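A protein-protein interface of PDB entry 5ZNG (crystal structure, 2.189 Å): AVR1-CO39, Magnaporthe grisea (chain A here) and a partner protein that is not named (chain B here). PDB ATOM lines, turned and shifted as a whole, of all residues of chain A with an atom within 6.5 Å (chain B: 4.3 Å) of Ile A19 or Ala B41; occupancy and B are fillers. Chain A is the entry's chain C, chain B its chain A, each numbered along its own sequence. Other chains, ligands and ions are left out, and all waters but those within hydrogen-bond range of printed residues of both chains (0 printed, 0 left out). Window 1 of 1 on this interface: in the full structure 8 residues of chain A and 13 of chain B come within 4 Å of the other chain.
The backbone carbonyl oxygen (O) of Ser B42 is in hydrogen-bond range of the backbone NH (N) of Ala A2, 3.3 Å away.
O of Val B46 sits at hydrogen-bond distance from OG1 of Thr A21 (2.7 Å).
The backbone carbonyl oxygen (O) of Val B46 sits close to the indole nitrogen (NE1) of Trp A3 (3.1 Å).
N of Val B49 lies within hydrogen-bond range of O of Ile A19, at 2.9 Å.
NH1 of Arg A10 is in hydrogen-bond range of OH of Tyr A20 (3.4 Å).
N of Ile A8 sits at hydrogen-bond distance from O of Tyr A20 (2.7 Å).
O of Asn A18 is in hydrogen-bond range of N of Arg A10 (3.0 Å).
The backbone carbonyl oxygen (O) of Leu B39 lies within hydrogen-bond range of the side-chain hydroxyl (OG) of Ser B42 (2.6 Å).
Among the printed residues, pairs that only touch across the chains: Trp A3 with Ala B41 (3.8 Å), Trp A3 with Ser B42 (3.9 Å), Trp A3 with Val B43 (3.5 Å), Ile A7 with Ala B41 (3.7 Å), Asn A17 with Met B37 (3.5 Å), Asn A18 with Met B37 (3.6 Å), Asn A18 with Val B49 (3.3 Å), Ile A19 with Met B37 (3.3 Å), Ile A19 with Ala B38 (3.8 Å), Ile A19 with Ala B41 (3.7 Å), Ile A19 with Ser B48 (3.3 Å), Tyr A20 with Ser B48 (3.6 Å) and Thr A21 with Ala B41 (3.5 Å).
Ile A19 touches just these residues of chain B: Met B37, Ala B38, Ala B41, Ser B48 and Val B49.
Of the printed residues of chain B, Thr A21 touches Ala B41 and Val B46.
Ala B41 touches just these residues of chain A: Trp A3 (3.8 Å), Ile A7 (3.7 Å), Ile A19 (3.7 Å) and Thr A21 (3.5 Å).
Of the printed residues of chain A, Val B49 touches Asn A18 (3.3 Å) and Ile A19 (2.9 Å).
The nearest residue of chain A that does not touch Ala B41 is Ala A2 (5.3 Å).
Hydrophobic or aromatic side chains of chain A within 4 Å of the printed part of chain B: Trp A3, Ile A7, Ile A19 and Tyr A20.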
ATOM      1  N   ALA A   2     -17.478   1.621 -15.726  1.00  0.00           N
ATOM      2  CA  ALA A   2     -16.303   2.401 -16.106  1.00  0.00           C
ATOM      3  C   ALA A   2     -15.646   1.812 -17.355  1.00  0.00           C
ATOM      4  O   ALA A   2     -15.349   0.617 -17.428  1.00  0.00           O
ATOM      5  CB  ALA A   2     -15.305   2.478 -14.952  1.00  0.00           C
ATOM      6  N   TRP A   3     -15.418   2.677 -18.343  1.00  0.00           N
ATOM      7  CA  TRP A   3     -14.979   2.253 -19.659  1.00  0.00           C
ATOM      8  C   TRP A   3     -13.510   2.544 -19.940  1.00  0.00           C
ATOM      9  O   TRP A   3     -12.955   1.964 -20.876  1.00  0.00           O
ATOM     10  CB  TRP A   3     -15.861   2.919 -20.730  1.00  0.00           C
ATOM     11  CG  TRP A   3     -15.647   4.403 -20.877  1.00  0.00           C
ATOM     12  CD1 TRP A   3     -15.835   5.371 -19.923  1.00  0.00           C
ATOM     13  CD2 TRP A   3     -15.202   5.083 -22.057  1.00  0.00           C
ATOM     14  NE1 TRP A   3     -15.517   6.612 -20.440  1.00  0.00           N
ATOM     15  CE2 TRP A   3     -15.125   6.460 -21.747  1.00  0.00           C
ATOM     16  CE3 TRP A   3     -14.859   4.659 -23.347  1.00  0.00           C
ATOM     17  CZ2 TRP A   3     -14.714   7.414 -22.684  1.00  0.00           C
ATOM     18  CZ3 TRP A   3     -14.453   5.607 -24.271  1.00  0.00           C
ATOM     19  CH2 TRP A   3     -14.386   6.969 -23.936  1.00  0.00           C
ATOM     20  N   LYS A   4     -12.871   3.413 -19.163  1.00  0.00           N
ATOM     21  CA  LYS A   4     -11.448   3.696 -19.291  1.00  0.00           C
ATOM     22  C   LYS A   4     -10.767   3.472 -17.945  1.00  0.00           C
ATOM     23  O   LYS A   4     -11.414   3.490 -16.893  1.00  0.00           O
ATOM     24  CB  LYS A   4     -11.199   5.131 -19.787  1.00  0.00           C
ATOM     25  CG  LYS A   4     -11.459   5.325 -21.285  1.00  0.00           C
ATOM     26  CD  LYS A   4     -10.871   6.632 -21.785  1.00  0.00           C
ATOM     27  CE  LYS A   4     -10.774   6.665 -23.306  1.00  0.00           C
ATOM     28  NZ  LYS A   4      -9.977   7.835 -23.789  1.00  0.00           N
ATOM     29  N   ILE A   7      -9.317   7.894 -13.803  1.00  0.00           N
ATOM     30  CA  ILE A   7     -10.036   9.137 -13.557  1.00  0.00           C
ATOM     31  C   ILE A   7      -9.016  10.191 -13.140  1.00  0.00           C
ATOM     32  O   ILE A   7      -8.235   9.962 -12.208  1.00  0.00           O
ATOM     33  CB  ILE A   7     -11.094   8.955 -12.454  1.00  0.00           C
ATOM     34  CG1 ILE A   7     -12.222   8.068 -12.954  1.00  0.00           C
ATOM     35  CG2 ILE A   7     -11.653  10.302 -12.055  1.00  0.00           C
ATOM     36  CD1 ILE A   7     -12.904   8.623 -14.181  1.00  0.00           C
ATOM     37  N   ILE A   8      -9.032  11.342 -13.806  1.00  0.00           N
ATOM     38  CA  ILE A   8      -8.156  12.462 -13.467  1.00  0.00           C
ATOM     39  C   ILE A   8      -9.018  13.550 -12.842  1.00  0.00           C
ATOM     40  O   ILE A   8      -9.962  14.036 -13.476  1.00  0.00           O
ATOM     41  CB  ILE A   8      -7.421  13.024 -14.693  1.00  0.00           C
ATOM     42  CG1 ILE A   8      -6.664  11.934 -15.470  1.00  0.00           C
ATOM     43  CG2 ILE A   8      -6.511  14.145 -14.252  1.00  0.00           C
ATOM     44  CD1 ILE A   8      -5.708  11.106 -14.602  1.00  0.00           C
ATOM     45  N   GLN A   9      -8.694  13.947 -11.619  1.00  0.00           N
ATOM     46  CA  GLN A   9      -9.388  15.042 -10.961  1.00  0.00           C
ATOM     47  C   GLN A   9      -8.587  16.324 -11.115  1.00  0.00           C
ATOM     48  O   GLN A   9      -7.352  16.310 -11.053  1.00  0.00           O
ATOM     49  CB  GLN A   9      -9.602  14.737  -9.478  1.00  0.00           C
ATOM     50  CG  GLN A   9     -10.302  13.411  -9.265  1.00  0.00           C
ATOM     51  CD  GLN A   9     -10.676  13.204  -7.836  1.00  0.00           C
ATOM     52  OE1 GLN A   9     -11.643  13.782  -7.352  1.00  0.00           O
ATOM     53  NE2 GLN A   9      -9.888  12.407  -7.127  1.00  0.00           N
ATOM     54  N   ARG A  10      -9.294  17.433 -11.296  1.00  0.00           N
ATOM     55  CA  ARG A  10      -8.664  18.737 -11.455  1.00  0.00           C
ATOM     56  C   ARG A  10      -9.118  19.660 -10.335  1.00  0.00           C
ATOM     57  O   ARG A  10     -10.299  19.998 -10.265  1.00  0.00           O
ATOM     58  CB  ARG A  10      -9.016  19.345 -12.803  1.00  0.00           C
ATOM     59  CG  ARG A  10      -8.269  20.602 -13.081  1.00  0.00           C
ATOM     60  CD  ARG A  10      -8.731  21.158 -14.391  1.00  0.00           C
ATOM     61  NE  ARG A  10      -8.196  22.482 -14.650  1.00  0.00           N
ATOM     62  CZ  ARG A  10      -8.740  23.324 -15.517  1.00  0.00           C
ATOM     63  NH1 ARG A  10      -9.828  22.957 -16.180  1.00  0.00           N
ATOM     64  NH2 ARG A  10      -8.201  24.522 -15.722  1.00  0.00           N
ATOM     65  N   VAL A  16     -12.706  20.308  -6.493  1.00  0.00           N
ATOM     66  CA  VAL A  16     -12.708  19.520  -7.717  1.00  0.00           C
ATOM     67  C   VAL A  16     -14.035  19.793  -8.410  1.00  0.00           C
ATOM     68  O   VAL A  16     -15.069  19.287  -7.987  1.00  0.00           O
ATOM     69  CB  VAL A  16     -12.544  18.023  -7.445  1.00  0.00           C
ATOM     70  CG1 VAL A  16     -12.603  17.219  -8.787  1.00  0.00           C
ATOM     71  CG2 VAL A  16     -11.272  17.756  -6.710  1.00  0.00           C
ATOM     72  N   ASN A  17     -14.020  20.558  -9.496  1.00  0.00           N
ATOM     73  CA  ASN A  17     -15.234  20.737 -10.286  1.00  0.00           C
ATOM     74  C   ASN A  17     -15.059  20.205 -11.702  1.00  0.00           C
ATOM     75  O   ASN A  17     -15.910  20.466 -12.557  1.00  0.00           O
ATOM     76  CB  ASN A  17     -15.667  22.212 -10.306  1.00  0.00           C
ATOM     77  CG  ASN A  17     -16.052  22.742  -8.907  1.00  0.00           C
ATOM     78  OD1 ASN A  17     -15.567  23.790  -8.479  1.00  0.00           O
ATOM     79  ND2 ASN A  17     -16.920  22.016  -8.199  1.00  0.00           N
ATOM     80  N   ASN A  18     -13.983  19.458 -11.963  1.00  0.00           N
ATOM     81  CA  ASN A  18     -13.721  18.864 -13.269  1.00  0.00           C
ATOM     82  C   ASN A  18     -13.035  17.521 -13.066  1.00  0.00           C
ATOM     83  O   ASN A  18     -12.071  17.442 -12.301  1.00  0.00           O
ATOM     84  CB  ASN A  18     -12.827  19.778 -14.139  1.00  0.00           C
ATOM     85  CG  ASN A  18     -13.439  21.152 -14.381  1.00  0.00           C
ATOM     86  OD1 ASN A  18     -13.401  22.026 -13.513  1.00  0.00           O
ATOM     87  ND2 ASN A  18     -14.014  21.344 -15.566  1.00  0.00           N
ATOM     88  N   ILE A  19     -13.524  16.473 -13.744  1.00  0.00           N
ATOM     89  CA  ILE A  19     -12.795  15.209 -13.850  1.00  0.00           C
ATOM     90  C   ILE A  19     -12.775  14.749 -15.308  1.00  0.00           C
ATOM     91  O   ILE A  19     -13.659  15.089 -16.098  1.00  0.00           O
ATOM     92  CB  ILE A  19     -13.381  14.094 -12.957  1.00  0.00           C
ATOM     93  CG1 ILE A  19     -14.704  13.620 -13.503  1.00  0.00           C
ATOM     94  CG2 ILE A  19     -13.519  14.538 -11.479  1.00  0.00           C
ATOM     95  CD1 ILE A  19     -15.349  12.576 -12.613  1.00  0.00           C
ATOM     96  N   TYR A  20     -11.760  13.944 -15.649  1.00  0.00           N
ATOM     97  CA  TYR A  20     -11.462  13.535 -17.021  1.00  0.00           C
ATOM     98  C   TYR A  20     -11.135  12.050 -17.041  1.00  0.00           C
ATOM     99  O   TYR A  20     -10.472  11.549 -16.130  1.00  0.00           O
ATOM    100  CB  TYR A  20     -10.274  14.344 -17.597  1.00  0.00           C
ATOM    101  CG  TYR A  20     -10.477  15.835 -17.474  1.00  0.00           C
ATOM    102  CD1 TYR A  20     -10.106  16.505 -16.314  1.00  0.00           C
ATOM    103  CD2 TYR A  20     -11.091  16.570 -18.497  1.00  0.00           C
ATOM    104  CE1 TYR A  20     -10.322  17.869 -16.168  1.00  0.00           C
ATOM    105  CE2 TYR A  20     -11.313  17.948 -18.365  1.00  0.00           C
ATOM    106  CZ  TYR A  20     -10.913  18.585 -17.190  1.00  0.00           C
ATOM    107  OH  TYR A  20     -11.097  19.937 -17.002  1.00  0.00           O
ATOM    108  N   THR A  21     -11.612  11.335 -18.057  1.00  0.00           N
ATOM    109  CA  THR A  21     -11.285   9.918 -18.178  1.00  0.00           C
ATOM    110  C   THR A  21     -10.058   9.757 -19.062  1.00  0.00           C
ATOM    111  O   THR A  21      -9.809  10.586 -19.945  1.00  0.00           O
ATOM    112  CB  THR A  21     -12.438   9.133 -18.782  1.00  0.00           C
ATOM    113  OG1 THR A  21     -12.797   9.734 -20.034  1.00  0.00           O
ATOM    114  CG2 THR A  21     -13.678   9.130 -17.839  1.00  0.00           C
ATOM    115  N   MET B  37     -20.085  12.882 -10.031  1.00  0.00           N
ATOM    116  CA  MET B  37     -19.164  13.055 -11.150  1.00  0.00           C
ATOM    117  C   MET B  37     -18.526  11.732 -11.527  1.00  0.00           C
ATOM    118  O   MET B  37     -18.457  11.373 -12.708  1.00  0.00           O
ATOM    119  CB  MET B  37     -18.089  14.071 -10.799  1.00  0.00           C
ATOM    120  CG  MET B  37     -18.558  15.495 -10.894  1.00  0.00           C
ATOM    121  SD  MET B  37     -17.206  16.582 -10.430  1.00  0.00           S
ATOM    122  CE  MET B  37     -16.634  17.078 -12.024  1.00  0.00           C
ATOM    123  N   ALA B  38     -18.056  10.984 -10.524  1.00  0.00           N
ATOM    124  CA  ALA B  38     -17.450   9.684 -10.797  1.00  0.00           C
ATOM    125  C   ALA B  38     -18.441   8.741 -11.468  1.00  0.00           C
ATOM    126  O   ALA B  38     -18.067   7.975 -12.365  1.00  0.00           O
ATOM    127  CB  ALA B  38     -16.916   9.076  -9.503  1.00  0.00           C
ATOM    128  N   LEU B  39     -19.719   8.801 -11.067  1.00  0.00           N
ATOM    129  CA  LEU B  39     -20.738   7.972 -11.713  1.00  0.00           C
ATOM    130  C   LEU B  39     -20.883   8.325 -13.182  1.00  0.00           C
ATOM    131  O   LEU B  39     -20.858   7.447 -14.053  1.00  0.00           O
ATOM    132  CB  LEU B  39     -22.083   8.138 -11.018  1.00  0.00           C
ATOM    133  CG  LEU B  39     -22.246   7.224  -9.816  1.00  0.00           C
ATOM    134  CD1 LEU B  39     -23.422   7.707  -9.027  1.00  0.00           C
ATOM    135  CD2 LEU B  39     -22.448   5.794 -10.295  1.00  0.00           C
ATOM    136  N   ALA B  40     -21.088   9.611 -13.472  1.00  0.00           N
ATOM    137  CA  ALA B  40     -21.173  10.044 -14.860  1.00  0.00           C
ATOM    138  C   ALA B  40     -19.936   9.631 -15.641  1.00  0.00           C
ATOM    139  O   ALA B  40     -20.040   9.150 -16.773  1.00  0.00           O
ATOM    140  CB  ALA B  40     -21.357  11.556 -14.924  1.00  0.00           C
ATOM    141  N   ALA B  41     -18.751   9.802 -15.048  1.00  0.00           N
ATOM    142  CA  ALA B  41     -17.517   9.455 -15.748  1.00  0.00           C
ATOM    143  C   ALA B  41     -17.433   7.978 -16.091  1.00  0.00           C
ATOM    144  O   ALA B  41     -16.659   7.609 -16.980  1.00  0.00           O
ATOM    145  CB  ALA B  41     -16.301   9.834 -14.906  1.00  0.00           C
ATOM    146  N   SER B  42     -18.192   7.118 -15.407  1.00  0.00           N
ATOM    147  CA  SER B  42     -18.115   5.687 -15.675  1.00  0.00           C
ATOM    148  C   SER B  42     -18.953   5.272 -16.877  1.00  0.00           C
ATOM    149  O   SER B  42     -18.898   4.106 -17.282  1.00  0.00           O
ATOM    150  CB  SER B  42     -18.577   4.898 -14.450  1.00  0.00           C
ATOM    151  OG  SER B  42     -19.995   5.012 -14.333  1.00  0.00           O
ATOM    152  N   VAL B  43     -19.720   6.178 -17.455  1.00  0.00           N
ATOM    153  CA  VAL B  43     -20.613   5.813 -18.554  1.00  0.00           C
ATOM    154  C   VAL B  43     -19.831   5.818 -19.860  1.00  0.00           C
ATOM    155  O   VAL B  43     -19.050   6.742 -20.134  1.00  0.00           O
ATOM    156  CB  VAL B  43     -21.810   6.768 -18.619  1.00  0.00           C
ATOM    157  CG1 VAL B  43     -22.645   6.510 -19.881  1.00  0.00           C
ATOM    158  CG2 VAL B  43     -22.669   6.629 -17.364  1.00  0.00           C
ATOM    159  N   VAL B  46     -17.823   8.815 -22.047  1.00  0.00           N
ATOM    160  CA  VAL B  46     -17.679  10.090 -21.350  1.00  0.00           C
ATOM    161  C   VAL B  46     -16.203  10.458 -21.239  1.00  0.00           C
ATOM    162  O   VAL B  46     -15.381   9.673 -20.743  1.00  0.00           O
ATOM    163  CB  VAL B  46     -18.355  10.039 -19.971  1.00  0.00           C
ATOM    164  CG1 VAL B  46     -18.003  11.286 -19.165  1.00  0.00           C
ATOM    165  CG2 VAL B  46     -19.878   9.923 -20.156  1.00  0.00           C
ATOM    166  N   SER B  48     -15.228  13.920 -20.122  1.00  0.00           N
ATOM    167  CA  SER B  48     -15.063  14.891 -19.044  1.00  0.00           C
ATOM    168  C   SER B  48     -16.411  15.161 -18.394  1.00  0.00           C
ATOM    169  O   SER B  48     -17.459  15.045 -19.032  1.00  0.00           O
ATOM    170  CB  SER B  48     -14.497  16.219 -19.546  1.00  0.00           C
ATOM    171  OG  SER B  48     -15.436  16.851 -20.407  1.00  0.00           O
ATOM    172  N   VAL B  49     -16.365  15.544 -17.122  1.00  0.00           N
ATOM    173  CA  VAL B  49     -17.537  15.934 -16.350  1.00  0.00           C
ATOM    174  C   VAL B  49     -17.193  17.213 -15.607  1.00  0.00           C
ATOM    175  O   VAL B  49     -16.096  17.340 -15.054  1.00  0.00           O
ATOM    176  CB  VAL B  49     -17.957  14.840 -15.349  1.00  0.00           C
ATOM    177  CG1 VAL B  49     -19.294  15.216 -14.681  1.00  0.00           C
ATOM    178  CG2 VAL B  49     -18.038  13.467 -16.045  1.00  0.00           C
